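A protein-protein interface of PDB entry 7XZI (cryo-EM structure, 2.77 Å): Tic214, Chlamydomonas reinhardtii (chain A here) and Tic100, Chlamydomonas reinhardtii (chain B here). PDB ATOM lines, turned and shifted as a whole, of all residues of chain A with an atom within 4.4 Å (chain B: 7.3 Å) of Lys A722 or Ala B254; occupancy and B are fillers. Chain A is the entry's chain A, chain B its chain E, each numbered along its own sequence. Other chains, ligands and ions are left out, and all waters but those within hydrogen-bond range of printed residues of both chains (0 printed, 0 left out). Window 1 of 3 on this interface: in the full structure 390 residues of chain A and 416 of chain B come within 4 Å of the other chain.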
ATOM      1  N   LYS A 718     -24.591  24.818  19.975  1.00  0.00           N
ATOM      2  CA  LYS A 718     -24.837  24.916  18.539  1.00  0.00           C
ATOM      3  C   LYS A 718     -25.601  23.699  18.030  1.00  0.00           C
ATOM      4  O   LYS A 718     -26.533  23.826  17.229  1.00  0.00           O
ATOM      5  CB  LYS A 718     -23.515  25.077  17.788  1.00  0.00           C
ATOM      6  CG  LYS A 718     -23.672  25.181  16.280  1.00  0.00           C
ATOM      7  CD  LYS A 718     -22.336  25.401  15.590  1.00  0.00           C
ATOM      8  CE  LYS A 718     -22.505  25.521  14.084  1.00  0.00           C
ATOM      9  NZ  LYS A 718     -23.047  24.273  13.478  1.00  0.00           N
ATOM     10  N   ALA A 719     -25.218  22.506  18.489  1.00  0.00           N
ATOM     11  CA  ALA A 719     -25.905  21.287  18.071  1.00  0.00           C
ATOM     12  C   ALA A 719     -27.354  21.279  18.539  1.00  0.00           C
ATOM     13  O   ALA A 719     -28.253  20.883  17.790  1.00  0.00           O
ATOM     14  CB  ALA A 719     -25.163  20.059  18.597  1.00  0.00           C
ATOM     15  N   LEU A 720     -27.600  21.709  19.780  1.00  0.00           N
ATOM     16  CA  LEU A 720     -28.969  21.744  20.287  1.00  0.00           C
ATOM     17  C   LEU A 720     -29.810  22.792  19.571  1.00  0.00           C
ATOM     18  O   LEU A 720     -31.018  22.600  19.399  1.00  0.00           O
ATOM     19  CB  LEU A 720     -28.970  21.997  21.794  1.00  0.00           C
ATOM     20  CG  LEU A 720     -28.494  20.838  22.673  1.00  0.00           C
ATOM     21  CD1 LEU A 720     -28.611  21.194  24.144  1.00  0.00           C
ATOM     22  CD2 LEU A 720     -29.287  19.582  22.361  1.00  0.00           C
ATOM     23  N   MET A 721     -29.201  23.904  19.154  1.00  0.00           N
ATOM     24  CA  MET A 721     -29.942  24.898  18.385  1.00  0.00           C
ATOM     25  C   MET A 721     -30.234  24.422  16.967  1.00  0.00           C
ATOM     26  O   MET A 721     -31.321  24.685  16.444  1.00  0.00           O
ATOM     27  CB  MET A 721     -29.174  26.219  18.348  1.00  0.00           C
ATOM     28  CG  MET A 721     -29.230  27.004  19.648  1.00  0.00           C
ATOM     29  SD  MET A 721     -30.881  27.643  19.987  1.00  0.00           S
ATOM     30  CE  MET A 721     -31.141  28.676  18.547  1.00  0.00           C
ATOM     31  N   LYS A 722     -29.284  23.728  16.336  1.00  0.00           N
ATOM     32  CA  LYS A 722     -29.514  23.205  14.993  1.00  0.00           C
ATOM     33  C   LYS A 722     -30.595  22.130  15.001  1.00  0.00           C
ATOM     34  O   LYS A 722     -31.533  22.173  14.197  1.00  0.00           O
ATOM     35  CB  LYS A 722     -28.211  22.651  14.415  1.00  0.00           C
ATOM     36  CG  LYS A 722     -27.147  23.704  14.146  1.00  0.00           C
ATOM     37  CD  LYS A 722     -27.328  24.347  12.783  1.00  0.00           C
ATOM     38  CE  LYS A 722     -27.068  23.342  11.672  1.00  0.00           C
ATOM     39  NZ  LYS A 722     -27.121  23.959  10.318  1.00  0.00           N
ATOM     40  N   ARG A 723     -30.477  21.156  15.900  1.00  0.00           N
ATOM     41  CA  ARG A 723     -31.470  20.102  16.052  1.00  0.00           C
ATOM     42  C   ARG A 723     -31.754  19.887  17.530  1.00  0.00           C
ATOM     43  O   ARG A 723     -30.843  19.924  18.362  1.00  0.00           O
ATOM     44  CB  ARG A 723     -31.010  18.795  15.390  1.00  0.00           C
ATOM     45  CG  ARG A 723     -29.667  18.269  15.866  1.00  0.00           C
ATOM     46  CD  ARG A 723     -28.801  17.842  14.689  1.00  0.00           C
ATOM     47  NE  ARG A 723     -29.541  17.052  13.715  1.00  0.00           N
ATOM     48  CZ  ARG A 723     -29.601  15.724  13.712  1.00  0.00           C
ATOM     49  NH1 ARG A 723     -28.977  15.002  14.627  1.00  0.00           N
ATOM     50  NH2 ARG A 723     -30.305  15.110  12.766  1.00  0.00           N
ATOM     51  N   SER B 251     -25.584  16.670   3.473  1.00  0.00           N
ATOM     52  CA  SER B 251     -26.148  17.659   2.562  1.00  0.00           C
ATOM     53  C   SER B 251     -27.630  17.922   2.807  1.00  0.00           C
ATOM     54  O   SER B 251     -28.276  18.552   1.963  1.00  0.00           O
ATOM     55  CB  SER B 251     -25.932  17.229   1.104  1.00  0.00           C
ATOM     56  OG  SER B 251     -24.552  17.116   0.802  1.00  0.00           O
ATOM     57  N   GLU B 252     -28.188  17.463   3.924  1.00  0.00           N
ATOM     58  CA  GLU B 252     -29.597  17.681   4.206  1.00  0.00           C
ATOM     59  C   GLU B 252     -29.809  19.059   4.832  1.00  0.00           C
ATOM     60  O   GLU B 252     -28.925  19.620   5.486  1.00  0.00           O
ATOM     61  CB  GLU B 252     -30.132  16.581   5.119  1.00  0.00           C
ATOM     62  CG  GLU B 252     -31.649  16.477   5.147  1.00  0.00           C
ATOM     63  CD  GLU B 252     -32.138  15.261   5.905  1.00  0.00           C
ATOM     64  OE1 GLU B 252     -31.311  14.601   6.568  1.00  0.00           O
ATOM     65  OE2 GLU B 252     -33.349  14.961   5.832  1.00  0.00           O
ATOM     66  N   TRP B 253     -31.003  19.606   4.626  1.00  0.00           N
ATOM     67  CA  TRP B 253     -31.322  20.939   5.116  1.00  0.00           C
ATOM     68  C   TRP B 253     -31.484  20.936   6.631  1.00  0.00           C
ATOM     69  O   TRP B 253     -32.006  19.987   7.222  1.00  0.00           O
ATOM     70  CB  TRP B 253     -32.600  21.460   4.461  1.00  0.00           C
ATOM     71  CG  TRP B 253     -32.821  22.929   4.655  1.00  0.00           C
ATOM     72  CD1 TRP B 253     -32.415  23.932   3.825  1.00  0.00           C
ATOM     73  CD2 TRP B 253     -33.502  23.564   5.747  1.00  0.00           C
ATOM     74  NE1 TRP B 253     -32.799  25.150   4.328  1.00  0.00           N
ATOM     75  CE2 TRP B 253     -33.466  24.952   5.508  1.00  0.00           C
ATOM     76  CE3 TRP B 253     -34.135  23.094   6.902  1.00  0.00           C
ATOM     77  CZ2 TRP B 253     -34.041  25.876   6.379  1.00  0.00           C
ATOM     78  CZ3 TRP B 253     -34.705  24.013   7.766  1.00  0.00           C
ATOM     79  CH2 TRP B 253     -34.653  25.387   7.500  1.00  0.00           C
ATOM     80  N   ALA B 254     -31.032  22.020   7.257  1.00  0.00           N
ATOM     81  CA  ALA B 254     -31.119  22.186   8.700  1.00  0.00           C
ATOM     82  C   ALA B 254     -31.351  23.655   9.005  1.00  0.00           C
ATOM     83  O   ALA B 254     -30.931  24.520   8.228  1.00  0.00           O
ATOM     84  CB  ALA B 254     -29.846  21.694   9.404  1.00  0.00           C
ATOM     85  N   PRO B 255     -32.018  23.972  10.116  1.00  0.00           N
ATOM     86  CA  PRO B 255     -32.201  25.380  10.484  1.00  0.00           C
ATOM     87  C   PRO B 255     -30.868  26.054  10.771  1.00  0.00           C
ATOM     88  O   PRO B 255     -29.913  25.425  11.229  1.00  0.00           O
ATOM     89  CB  PRO B 255     -33.074  25.310  11.742  1.00  0.00           C
ATOM     90  CG  PRO B 255     -33.743  23.982  11.668  1.00  0.00           C
ATOM     91  CD  PRO B 255     -32.751  23.069  11.018  1.00  0.00           C
ATOM     92  N   GLU B 256     -30.811  27.352  10.489  1.00  0.00           N
ATOM     93  CA  GLU B 256     -29.590  28.107  10.709  1.00  0.00           C
ATOM     94  C   GLU B 256     -29.326  28.303  12.199  1.00  0.00           C
ATOM     95  O   GLU B 256     -30.222  28.202  13.042  1.00  0.00           O
ATOM     96  CB  GLU B 256     -29.660  29.471  10.027  1.00  0.00           C
ATOM     97  CG  GLU B 256     -29.729  29.422   8.518  1.00  0.00           C
ATOM     98  CD  GLU B 256     -29.414  30.763   7.891  1.00  0.00           C
ATOM     99  OE1 GLU B 256     -28.491  31.444   8.386  1.00  0.00           O
ATOM    100  OE2 GLU B 256     -30.095  31.140   6.915  1.00  0.00           O
ATOM    101  N   TYR B 257     -28.068  28.597  12.510  1.00  0.00           N
ATOM    102  CA  TYR B 257     -27.647  28.989  13.848  1.00  0.00           C
ATOM    103  C   TYR B 257     -27.201  30.440  13.786  1.00  0.00           C
ATOM    104  O   TYR B 257     -26.265  30.771  13.051  1.00  0.00           O
ATOM    105  CB  TYR B 257     -26.518  28.093  14.357  1.00  0.00           C
ATOM    106  CG  TYR B 257     -25.783  28.659  15.548  1.00  0.00           C
ATOM    107  CD1 TYR B 257     -26.334  28.602  16.818  1.00  0.00           C
ATOM    108  CD2 TYR B 257     -24.536  29.251  15.402  1.00  0.00           C
ATOM    109  CE1 TYR B 257     -25.667  29.119  17.909  1.00  0.00           C
ATOM    110  CE2 TYR B 257     -23.861  29.770  16.487  1.00  0.00           C
ATOM    111  CZ  TYR B 257     -24.431  29.701  17.738  1.00  0.00           C
ATOM    112  OH  TYR B 257     -23.762  30.216  18.823  1.00  0.00           O
ATOM    113  N   VAL B 258     -27.867  31.302  14.553  1.00  0.00           N
ATOM    114  CA  VAL B 258     -27.583  32.730  14.547  1.00  0.00           C
ATOM    115  C   VAL B 258     -27.128  33.244  15.900  1.00  0.00           C
ATOM    116  O   VAL B 258     -26.752  34.416  16.007  1.00  0.00           O
ATOM    117  CB  VAL B 258     -28.799  33.542  14.055  1.00  0.00           C
ATOM    118  CG1 VAL B 258     -29.135  33.184  12.618  1.00  0.00           C
ATOM    119  CG2 VAL B 258     -29.994  33.305  14.961  1.00  0.00           C
ATOM    120  N   HIS B 278     -35.486  31.521   9.415  1.00  0.00           N
ATOM    121  CA  HIS B 278     -34.933  30.201   9.142  1.00  0.00           C
ATOM    122  C   HIS B 278     -34.152  29.632  10.322  1.00  0.00           C
ATOM    123  O   HIS B 278     -33.358  28.705  10.140  1.00  0.00           O
ATOM    124  CB  HIS B 278     -34.048  30.251   7.896  1.00  0.00           C
ATOM    125  CG  HIS B 278     -34.815  30.356   6.614  1.00  0.00           C
ATOM    126  ND1 HIS B 278     -34.306  30.972   5.490  1.00  0.00           N
ATOM    127  CD2 HIS B 278     -36.049  29.915   6.275  1.00  0.00           C
ATOM    128  CE1 HIS B 278     -35.197  30.911   4.516  1.00  0.00           C
ATOM    129  NE2 HIS B 278     -36.262  30.274   4.966  1.00  0.00           N
ATOM    130  N   ASN B 280     -34.124  28.958  14.966  1.00  0.00           N
ATOM    131  CA  ASN B 280     -34.920  28.684  16.154  1.00  0.00           C
ATOM    132  C   ASN B 280     -34.765  29.786  17.197  1.00  0.00           C
ATOM    133  O   ASN B 280     -34.903  29.541  18.398  1.00  0.00           O
ATOM    134  CB  ASN B 280     -34.552  27.326  16.750  1.00  0.00           C
ATOM    135  CG  ASN B 280     -34.957  26.168  15.856  1.00  0.00           C
ATOM    136  OD1 ASN B 280     -35.888  26.279  15.058  1.00  0.00           O
ATOM    137  ND2 ASN B 280     -34.261  25.045  15.990  1.00  0.00           N
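Hydrophobic or aromatic side chains of chain A within 4 Å of the printed part of chain B: Met A721.
Of the 10 printed residues of chain B, 3 touch a printed residue of chain A.
Hydrophobic or aromatic side chains of chain B that line the printed part of chain A: Ala B254 and Pro B255.
Among the printed residues, 3 pairs touch across the chains.
ND2 of Asn B280 is in hydrogen-bond range of O of Met A721, 3.0 Å away.
The backbone carbonyl oxygen (O) of Pro B255 sits close to the side-chain amino group (NZ) of Lys A722 (3.3 Å).
Lys A722 touches Ala B254 (NZ to CB, 3.7 Å).
Of the printed residues of chain B, Met A721 touches Asn B280.
Lys A722 touches two residues of chain B.
Of the printed residues of chain A, Ala B254 touches Lys A722 (3.7 Å).
Of the printed residues of chain A, Pro B255 touches Lys A722.
Printed residues of chain A within 4 Å of Asn B280: Met A721 (3.0 Å).
The nearest residue of chain B that does not touch Lys A722 is Tyr B257 (4.1 Å).
The nearest printed residue of chain A that does not touch Asn B280 is Lys A722 (4.3 Å).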
